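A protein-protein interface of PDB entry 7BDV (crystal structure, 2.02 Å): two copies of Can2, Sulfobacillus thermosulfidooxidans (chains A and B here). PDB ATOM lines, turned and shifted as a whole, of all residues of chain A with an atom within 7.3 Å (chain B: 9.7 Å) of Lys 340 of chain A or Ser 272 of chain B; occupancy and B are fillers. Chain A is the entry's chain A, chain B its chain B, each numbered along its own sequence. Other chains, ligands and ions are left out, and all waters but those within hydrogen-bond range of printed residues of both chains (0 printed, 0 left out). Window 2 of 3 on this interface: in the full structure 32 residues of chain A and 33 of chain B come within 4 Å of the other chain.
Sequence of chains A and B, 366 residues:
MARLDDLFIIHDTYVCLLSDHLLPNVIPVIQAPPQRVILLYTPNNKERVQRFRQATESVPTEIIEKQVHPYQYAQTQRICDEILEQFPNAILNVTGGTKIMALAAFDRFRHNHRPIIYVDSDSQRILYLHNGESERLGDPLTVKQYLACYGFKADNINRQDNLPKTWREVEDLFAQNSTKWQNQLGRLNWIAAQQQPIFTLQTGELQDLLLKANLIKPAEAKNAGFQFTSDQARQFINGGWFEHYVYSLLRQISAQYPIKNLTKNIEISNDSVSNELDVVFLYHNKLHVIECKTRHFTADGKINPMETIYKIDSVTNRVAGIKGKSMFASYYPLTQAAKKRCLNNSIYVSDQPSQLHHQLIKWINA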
ATOM      1  N   MET A 306      10.503   8.342 -13.602  1.00  0.00           N
ATOM      2  CA  MET A 306       9.577   9.058 -14.465  1.00  0.00           C
ATOM      3  C   MET A 306       9.999   8.950 -15.933  1.00  0.00           C
ATOM      4  O   MET A 306       9.163   8.692 -16.790  1.00  0.00           O
ATOM      5  CB  MET A 306       9.448  10.518 -14.017  1.00  0.00           C
ATOM      6  CG  MET A 306       8.681  10.711 -12.722  1.00  0.00           C
ATOM      7  SD  MET A 306       6.807  10.134 -12.870  1.00  0.00           S
ATOM      8  CE  MET A 306       5.635  11.435 -11.960  1.00  0.00           C
ATOM      9  N   ILE A 309       8.995   5.523 -17.171  1.00  0.00           N
ATOM     10  CA  ILE A 309       7.533   5.361 -17.389  1.00  0.00           C
ATOM     11  C   ILE A 309       7.136   5.907 -18.773  1.00  0.00           C
ATOM     12  O   ILE A 309       6.330   5.248 -19.455  1.00  0.00           O
ATOM     13  CB  ILE A 309       6.723   6.010 -16.253  1.00  0.00           C
ATOM     14  CG1 ILE A 309       7.007   5.324 -14.913  1.00  0.00           C
ATOM     15  CG2 ILE A 309       5.245   6.004 -16.608  1.00  0.00           C
ATOM     16  CD1 ILE A 309       6.551   6.124 -13.697  1.00  0.00           C
ATOM     17  N   THR A 335       7.872   6.096  -5.676  1.00  0.00           N
ATOM     18  CA  THR A 335       7.084   7.227  -5.118  1.00  0.00           C
ATOM     19  C   THR A 335       5.623   7.084  -5.555  1.00  0.00           C
ATOM     20  O   THR A 335       5.341   6.336  -6.557  1.00  0.00           O
ATOM     21  CB  THR A 335       7.671   8.572  -5.555  1.00  0.00           C
ATOM     22  OG1 THR A 335       6.803   9.572  -5.027  1.00  0.00           O
ATOM     23  CG2 THR A 335       7.803   8.717  -7.054  1.00  0.00           C
ATOM     24  N   GLN A 336       4.714   7.758  -4.850  1.00  0.00           N
ATOM     25  CA  GLN A 336       3.255   7.675  -5.123  1.00  0.00           C
ATOM     26  C   GLN A 336       2.976   8.231  -6.522  1.00  0.00           C
ATOM     27  O   GLN A 336       2.169   7.644  -7.240  1.00  0.00           O
ATOM     28  CB  GLN A 336       2.439   8.407  -4.056  1.00  0.00           C
ATOM     29  CG  GLN A 336       1.114   7.721  -3.772  1.00  0.00           C
ATOM     30  CD  GLN A 336       1.306   6.241  -3.551  1.00  0.00           C
ATOM     31  OE1 GLN A 336       1.948   5.815  -2.598  1.00  0.00           O
ATOM     32  NE2 GLN A 336       0.766   5.439  -4.454  1.00  0.00           N
ATOM     33  N   ALA A 337       3.641   9.321  -6.890  1.00  0.00           N
ATOM     34  CA  ALA A 337       3.489  10.021  -8.180  1.00  0.00           C
ATOM     35  C   ALA A 337       3.814   9.064  -9.337  1.00  0.00           C
ATOM     36  O   ALA A 337       3.069   9.070 -10.335  1.00  0.00           O
ATOM     37  CB  ALA A 337       4.390  11.225  -8.177  1.00  0.00           C
ATOM     38  N   ALA A 338       4.888   8.291  -9.225  1.00  0.00           N
ATOM     39  CA  ALA A 338       5.339   7.334 -10.265  1.00  0.00           C
ATOM     40  C   ALA A 338       4.271   6.255 -10.427  1.00  0.00           C
ATOM     41  O   ALA A 338       3.957   5.902 -11.590  1.00  0.00           O
ATOM     42  CB  ALA A 338       6.683   6.738  -9.912  1.00  0.00           C
ATOM     43  N   LYS A 339       3.689   5.792  -9.310  1.00  0.00           N
ATOM     44  CA  LYS A 339       2.623   4.757  -9.301  1.00  0.00           C
ATOM     45  C   LYS A 339       1.360   5.336  -9.940  1.00  0.00           C
ATOM     46  O   LYS A 339       0.696   4.621 -10.732  1.00  0.00           O
ATOM     47  CB  LYS A 339       2.367   4.219  -7.888  1.00  0.00           C
ATOM     48  CG  LYS A 339       3.380   3.190  -7.391  1.00  0.00           C
ATOM     49  CD  LYS A 339       3.336   2.953  -5.906  1.00  0.00           C
ATOM     50  CE  LYS A 339       4.180   1.773  -5.478  1.00  0.00           C
ATOM     51  NZ  LYS A 339       4.444   1.813  -4.022  1.00  0.00           N
ATOM     52  N   LYS A 340       1.035   6.593  -9.636  1.00  0.00           N
ATOM     53  CA  LYS A 340      -0.164   7.259 -10.194  1.00  0.00           C
ATOM     54  C   LYS A 340      -0.001   7.429 -11.716  1.00  0.00           C
ATOM     55  O   LYS A 340      -1.000   7.226 -12.438  1.00  0.00           O
ATOM     56  CB  LYS A 340      -0.428   8.570  -9.445  1.00  0.00           C
ATOM     57  CG  LYS A 340      -1.213   8.392  -8.143  1.00  0.00           C
ATOM     58  CD  LYS A 340      -1.029   9.519  -7.112  1.00  0.00           C
ATOM     59  N   ARG A 341       1.193   7.767 -12.210  1.00  0.00           N
ATOM     60  CA  ARG A 341       1.408   7.936 -13.674  1.00  0.00           C
ATOM     61  C   ARG A 341       1.237   6.571 -14.355  1.00  0.00           C
ATOM     62  O   ARG A 341       0.556   6.502 -15.420  1.00  0.00           O
ATOM     63  CB  ARG A 341       2.760   8.579 -13.996  1.00  0.00           C
ATOM     64  CG  ARG A 341       2.932   8.841 -15.492  1.00  0.00           C
ATOM     65  CD  ARG A 341       4.039   9.825 -15.801  1.00  0.00           C
ATOM     66  NE  ARG A 341       3.798  11.148 -15.234  1.00  0.00           N
ATOM     67  CZ  ARG A 341       3.104  12.136 -15.804  1.00  0.00           C
ATOM     68  NH1 ARG A 341       2.541  11.987 -16.995  1.00  0.00           N
ATOM     69  NH2 ARG A 341       2.979  13.283 -15.163  1.00  0.00           N
ATOM     70  N   CYS A 342       1.793   5.515 -13.762  1.00  0.00           N
ATOM     71  CA  CYS A 342       1.628   4.130 -14.257  1.00  0.00           C
ATOM     72  C   CYS A 342       0.145   3.769 -14.367  1.00  0.00           C
ATOM     73  O   CYS A 342      -0.272   3.285 -15.445  1.00  0.00           O
ATOM     74  CB  CYS A 342       2.365   3.142 -13.364  1.00  0.00           C
ATOM     75  SG  CYS A 342       4.148   3.256 -13.574  1.00  0.00           S
ATOM     76  N   LEU A 343      -0.636   3.992 -13.306  1.00  0.00           N
ATOM     77  CA  LEU A 343      -2.104   3.729 -13.314  1.00  0.00           C
ATOM     78  C   LEU A 343      -2.744   4.523 -14.459  1.00  0.00           C
ATOM     79  O   LEU A 343      -3.503   3.934 -15.240  1.00  0.00           O
ATOM     80  CB  LEU A 343      -2.730   4.104 -11.962  1.00  0.00           C
ATOM     81  CG  LEU A 343      -4.248   3.936 -11.879  1.00  0.00           C
ATOM     82  CD1 LEU A 343      -4.621   2.463 -12.025  1.00  0.00           C
ATOM     83  CD2 LEU A 343      -4.803   4.521 -10.582  1.00  0.00           C
ATOM     84  N   ASN A 344      -2.434   5.814 -14.555  1.00  0.00           N
ATOM     85  CA  ASN A 344      -2.972   6.710 -15.604  1.00  0.00           C
ATOM     86  C   ASN A 344      -2.636   6.167 -17.012  1.00  0.00           C
ATOM     87  O   ASN A 344      -3.442   6.360 -17.923  1.00  0.00           O
ATOM     88  CB  ASN A 344      -2.417   8.121 -15.431  1.00  0.00           C
ATOM     89  CG  ASN A 344      -3.126   9.112 -16.326  1.00  0.00           C
ATOM     90  OD1 ASN A 344      -4.321   9.330 -16.150  1.00  0.00           O
ATOM     91  ND2 ASN A 344      -2.416   9.680 -17.290  1.00  0.00           N
ATOM     92  N   ASN A 345      -1.484   5.511 -17.181  1.00  0.00           N
ATOM     93  CA  ASN A 345      -0.951   5.092 -18.508  1.00  0.00           C
ATOM     94  C   ASN A 345      -1.250   3.610 -18.781  1.00  0.00           C
ATOM     95  O   ASN A 345      -0.701   3.080 -19.763  1.00  0.00           O
ATOM     96  CB  ASN A 345       0.551   5.368 -18.594  1.00  0.00           C
ATOM     97  CG  ASN A 345       0.871   6.841 -18.747  1.00  0.00           C
ATOM     98  OD1 ASN A 345       0.003   7.709 -18.606  1.00  0.00           O
ATOM     99  ND2 ASN A 345       2.124   7.130 -19.033  1.00  0.00           N
ATOM    100  N   SER A 346      -2.058   2.975 -17.927  1.00  0.00           N
ATOM    101  CA  SER A 346      -2.425   1.534 -17.958  1.00  0.00           C
ATOM    102  C   SER A 346      -1.174   0.647 -17.872  1.00  0.00           C
ATOM    103  O   SER A 346      -1.161  -0.429 -18.494  1.00  0.00           O
ATOM    104  CB  SER A 346      -3.243   1.198 -19.194  1.00  0.00           C
ATOM    105  OG  SER A 346      -4.504   1.843 -19.169  1.00  0.00           O
ATOM    106  N   VAL A 349       2.131  -1.920 -12.082  1.00  0.00           N
ATOM    107  CA  VAL A 349       3.353  -1.532 -11.322  1.00  0.00           C
ATOM    108  C   VAL A 349       3.515  -2.439 -10.097  1.00  0.00           C
ATOM    109  O   VAL A 349       2.540  -2.676  -9.369  1.00  0.00           O
ATOM    110  CB  VAL A 349       3.413  -0.019 -11.008  1.00  0.00           C
ATOM    111  CG1 VAL A 349       2.191   0.506 -10.273  1.00  0.00           C
ATOM    112  CG2 VAL A 349       4.690   0.315 -10.266  1.00  0.00           C
ATOM    113  N   ARG B  51     -17.051  13.029 -17.654  1.00  0.00           N
ATOM    114  CA  ARG B  51     -16.254  13.803 -18.633  1.00  0.00           C
ATOM    115  C   ARG B  51     -17.173  14.523 -19.634  1.00  0.00           C
ATOM    116  O   ARG B  51     -16.918  15.703 -19.934  1.00  0.00           O
ATOM    117  CB  ARG B  51     -15.319  12.889 -19.421  1.00  0.00           C
ATOM    118  CG  ARG B  51     -14.178  12.338 -18.600  1.00  0.00           C
ATOM    119  CD  ARG B  51     -13.221  11.675 -19.555  1.00  0.00           C
ATOM    120  NE  ARG B  51     -12.112  11.085 -18.836  1.00  0.00           N
ATOM    121  CZ  ARG B  51     -11.092  10.466 -19.417  1.00  0.00           C
ATOM    122  NH1 ARG B  51     -11.055  10.342 -20.733  1.00  0.00           N
ATOM    123  NH2 ARG B  51     -10.118   9.966 -18.675  1.00  0.00           N
ATOM    124  N   TYR B 150     -10.750  14.444 -22.197  1.00  0.00           N
ATOM    125  CA  TYR B 150      -9.638  13.530 -21.830  1.00  0.00           C
ATOM    126  C   TYR B 150      -9.417  13.545 -20.314  1.00  0.00           C
ATOM    127  O   TYR B 150      -8.451  12.962 -19.835  1.00  0.00           O
ATOM    128  CB  TYR B 150      -8.414  13.893 -22.662  1.00  0.00           C
ATOM    129  CG  TYR B 150      -8.580  13.554 -24.119  1.00  0.00           C
ATOM    130  CD1 TYR B 150      -8.447  12.244 -24.555  1.00  0.00           C
ATOM    131  CD2 TYR B 150      -8.905  14.508 -25.058  1.00  0.00           C
ATOM    132  CE1 TYR B 150      -8.580  11.911 -25.886  1.00  0.00           C
ATOM    133  CE2 TYR B 150      -9.011  14.195 -26.406  1.00  0.00           C
ATOM    134  CZ  TYR B 150      -8.890  12.880 -26.816  1.00  0.00           C
ATOM    135  OH  TYR B 150      -9.078  12.525 -28.122  1.00  0.00           O
ATOM    136  N   GLY B 151     -10.340  14.135 -19.566  1.00  0.00           N
ATOM    137  CA  GLY B 151     -10.326  14.095 -18.095  1.00  0.00           C
ATOM    138  C   GLY B 151      -9.424  15.142 -17.493  1.00  0.00           C
ATOM    139  O   GLY B 151      -9.197  15.039 -16.285  1.00  0.00           O
ATOM    140  N   PHE B 152      -8.939  16.115 -18.267  1.00  0.00           N
ATOM    141  CA  PHE B 152      -7.935  17.101 -17.778  1.00  0.00           C
ATOM    142  C   PHE B 152      -8.578  18.465 -17.535  1.00  0.00           C
ATOM    143  O   PHE B 152      -9.483  18.847 -18.272  1.00  0.00           O
ATOM    144  CB  PHE B 152      -6.785  17.265 -18.767  1.00  0.00           C
ATOM    145  CG  PHE B 152      -5.821  16.123 -18.688  1.00  0.00           C
ATOM    146  CD1 PHE B 152      -4.856  16.089 -17.693  1.00  0.00           C
ATOM    147  CD2 PHE B 152      -5.949  15.046 -19.551  1.00  0.00           C
ATOM    148  CE1 PHE B 152      -3.982  15.020 -17.601  1.00  0.00           C
ATOM    149  CE2 PHE B 152      -5.050  13.988 -19.480  1.00  0.00           C
ATOM    150  CZ  PHE B 152      -4.090  13.961 -18.483  1.00  0.00           C
ATOM    151  N   LYS B 153      -8.085  19.163 -16.518  1.00  0.00           N
ATOM    152  CA  LYS B 153      -8.446  20.577 -16.235  1.00  0.00           C
ATOM    153  C   LYS B 153      -7.137  21.364 -16.097  1.00  0.00           C
ATOM    154  O   LYS B 153      -6.126  20.741 -15.739  1.00  0.00           O
ATOM    155  CB  LYS B 153      -9.360  20.655 -15.008  1.00  0.00           C
ATOM    156  CG  LYS B 153      -8.759  20.168 -13.702  1.00  0.00           C
ATOM    157  CD  LYS B 153      -9.807  19.875 -12.635  1.00  0.00           C
ATOM    158  CE  LYS B 153      -9.247  19.905 -11.229  1.00  0.00           C
ATOM    159  N   ILE B 268      -1.786  21.115 -16.481  1.00  0.00           N
ATOM    160  CA  ILE B 268      -3.045  20.320 -16.588  1.00  0.00           C
ATOM    161  C   ILE B 268      -2.944  19.100 -15.680  1.00  0.00           C
ATOM    162  O   ILE B 268      -1.884  18.472 -15.615  1.00  0.00           O
ATOM    163  CB  ILE B 268      -3.388  19.967 -18.048  1.00  0.00           C
ATOM    164  CG1 ILE B 268      -2.348  19.048 -18.688  1.00  0.00           C
ATOM    165  CG2 ILE B 268      -3.572  21.249 -18.847  1.00  0.00           C
ATOM    166  CD1 ILE B 268      -2.718  18.585 -20.076  1.00  0.00           C
ATOM    167  N   SER B 269      -4.041  18.769 -15.016  1.00  0.00           N
ATOM    168  CA  SER B 269      -4.148  17.602 -14.110  1.00  0.00           C
ATOM    169  C   SER B 269      -5.418  16.817 -14.442  1.00  0.00           C
ATOM    170  O   SER B 269      -6.369  17.431 -14.947  1.00  0.00           O
ATOM    171  CB  SER B 269      -4.134  18.050 -12.668  1.00  0.00           C
ATOM    172  OG  SER B 269      -5.372  18.652 -12.324  1.00  0.00           O
ATOM    173  N   ASN B 270      -5.420  15.518 -14.163  1.00  0.00           N
ATOM    174  CA  ASN B 270      -6.670  14.709 -14.136  1.00  0.00           C
ATOM    175  C   ASN B 270      -6.972  14.213 -12.719  1.00  0.00           C
ATOM    176  O   ASN B 270      -7.933  13.426 -12.579  1.00  0.00           O
ATOM    177  CB  ASN B 270      -6.629  13.543 -15.119  1.00  0.00           C
ATOM    178  CG  ASN B 270      -5.466  12.613 -14.866  1.00  0.00           C
ATOM    179  OD1 ASN B 270      -4.785  12.731 -13.846  1.00  0.00           O
ATOM    180  ND2 ASN B 270      -5.222  11.722 -15.802  1.00  0.00           N
ATOM    181  N   ASP B 271      -6.212  14.632 -11.715  1.00  0.00           N
ATOM    182  CA  ASP B 271      -6.448  14.195 -10.314  1.00  0.00           C
ATOM    183  C   ASP B 271      -5.571  12.993  -9.965  1.00  0.00           C
ATOM    184  O   ASP B 271      -5.415  12.749  -8.769  1.00  0.00           O
ATOM    185  N   SER B 272      -4.967  12.298 -10.943  1.00  0.00           N
ATOM    186  CA  SER B 272      -3.879  11.296 -10.712  1.00  0.00           C
ATOM    187  C   SER B 272      -2.486  11.827 -11.135  1.00  0.00           C
ATOM    188  O   SER B 272      -1.516  11.622 -10.394  1.00  0.00           O
ATOM    189  N   VAL B 273      -2.382  12.496 -12.292  1.00  0.00           N
ATOM    190  CA  VAL B 273      -1.110  13.064 -12.820  1.00  0.00           C
ATOM    191  C   VAL B 273      -1.292  14.555 -13.134  1.00  0.00           C
ATOM    192  O   VAL B 273      -2.432  14.991 -13.415  1.00  0.00           O
ATOM    193  CB  VAL B 273      -0.659  12.297 -14.074  1.00  0.00           C
ATOM    194  N   SER B 274      -0.188  15.302 -13.146  1.00  0.00           N
ATOM    195  CA  SER B 274      -0.105  16.672 -13.710  1.00  0.00           C
ATOM    196  C   SER B 274       0.977  16.715 -14.795  1.00  0.00           C
ATOM    197  O   SER B 274       2.023  16.094 -14.617  1.00  0.00           O
ATOM    198  CB  SER B 274       0.122  17.710 -12.636  1.00  0.00           C
ATOM    199  OG  SER B 274       1.226  17.361 -11.832  1.00  0.00           O
ATOM    200  N   ASN B 275       0.708  17.447 -15.875  1.00  0.00           N
ATOM    201  CA  ASN B 275       1.632  17.710 -17.008  1.00  0.00           C
ATOM    202  C   ASN B 275       1.727  19.224 -17.209  1.00  0.00           C
ATOM    203  O   ASN B 275       0.675  19.901 -17.102  1.00  0.00           O
ATOM    204  CB  ASN B 275       1.163  17.016 -18.290  1.00  0.00           C
ATOM    205  CG  ASN B 275       1.027  15.521 -18.102  1.00  0.00           C
ATOM    206  OD1 ASN B 275       1.998  14.883 -17.719  1.00  0.00           O
ATOM    207  ND2 ASN B 275      -0.159  14.964 -18.316  1.00  0.00           N
ATOM    208  N   ARG B 318      -2.014  11.024 -24.446  1.00  0.00           N
ATOM    209  CA  ARG B 318      -2.983  11.006 -23.327  1.00  0.00           C
ATOM    210  C   ARG B 318      -3.782  12.322 -23.295  1.00  0.00           C
ATOM    211  O   ARG B 318      -4.957  12.271 -22.972  1.00  0.00           O
ATOM    212  CB  ARG B 318      -2.245  10.728 -22.012  1.00  0.00           C
ATOM    213  CG  ARG B 318      -1.568   9.368 -21.965  1.00  0.00           C
ATOM    214  CD  ARG B 318      -2.489   8.171 -21.753  1.00  0.00           C
ATOM    215  NE  ARG B 318      -1.848   6.937 -22.207  1.00  0.00           N
ATOM    216  CZ  ARG B 318      -2.212   5.703 -21.859  1.00  0.00           C
ATOM    217  NH1 ARG B 318      -3.225   5.510 -21.029  1.00  0.00           N
ATOM    218  NH2 ARG B 318      -1.544   4.663 -22.333  1.00  0.00           N
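NH2 of Arg 341 of chain A sits at hydrogen-bond distance from O of Ser 274 of chain B, at 3.0 Å. OD1 of Asn 275 of chain B is in hydrogen-bond range of NH1 of Arg 341 of chain A. The side-chain amide nitrogen (ND2) of Asn 270 of chain B lies within hydrogen-bond range of the side-chain amide oxygen (OD1) of Asn 344 of chain A (2.6 Å). O of Asn 344 of chain A is in hydrogen-bond range of NH1 of Arg 318 of chain B, 3.2 Å away. The backbone carbonyl oxygen (O) of Asn 345 of chain A is in hydrogen-bond range of the guanidinium group (NH2) of Arg 318 of chain B, at 3.1 Å.
O of Arg 341 of chain A lies close to OD1 of Asn 345 of chain A (3.5 Å). The side-chain amide oxygen (OD1) of Asn 345 of chain A is in hydrogen-bond range of the side-chain amide nitrogen (ND2) of Asn 344 of chain A. The backbone carbonyl oxygen (O) of Ile 268 of chain B is in hydrogen-bond range of the backbone NH (N) of Asn 275 of chain B (2.8 Å). OD1 of Asn 270 of chain B sits at hydrogen-bond distance from N of Ser 272 of chain B. The backbone NH of Val 273 of chain B is in hydrogen-bond range of the side-chain amide oxygen of Asn 270 of chain B (2.9 Å).
Ser 272 of chain B touches Lys 340 of chain A (O to CB, 3.4 Å). NH2 of Arg 341 of chain A touches CB of Val 273 of chain B, at 3.9 Å.
Met 306 of chain A touches none of the printed residues of chain B. Gln 336 of chain A touches none of the printed residues of chain B. No residue of chain B comes within 4 Å of Ala 337 of chain A. Of chain B, only Ser 272 (3.4 Å) comes within 4 Å of Lys 340 of chain A. Printed residues of chain B within 4 Å of Asn 344 of chain A: Asn 270 and Arg 318. Printed residues of chain B within 4 Å of Asn 345 of chain A: Arg 318 (3.1 Å). Of the printed residues of chain A, Asn 270 of chain B touches Asn 344. No residue of chain A comes within 4 Å of Asp 271 of chain B. Of chain A, only Lys 340 (3.4 Å) comes within 4 Å of Ser 272 of chain B. Of the printed residues of chain A, Val 273 of chain B touches Arg 341 (3.9 Å). Printed residues of chain A within 4 Å of Asn 275 of chain B: Arg 341. The nearest residue of chain B that does not touch Lys 340 of chain A is Val 273 of chain B (5.2 Å). The nearest printed residue of chain A that does not touch Asn 270 of chain B is Lys 340 of chain A (6.8 Å).
Printed residues of chain B that touch a printed residue of chain A: Asn 270, Ser 272, Val 273, Ser 274, Asn 275 and Arg 318. Along chain B the printed residues that touch a printed residue of chain A span positions 270 to 318. Of the 15 printed residues of chain A, 4 touch a printed residue of chain B. Among the printed residues, 7 pairs touch across the chains. Among the printed residues, no Asp or Glu carboxylate lies within 4 Å of a Lys or Arg side-chain nitrogen of the other chain.
No position is printed for both chains. Of the 7 pairs that touch across the chains among the printed residues, none has its exchanged pair printed and touching as well.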
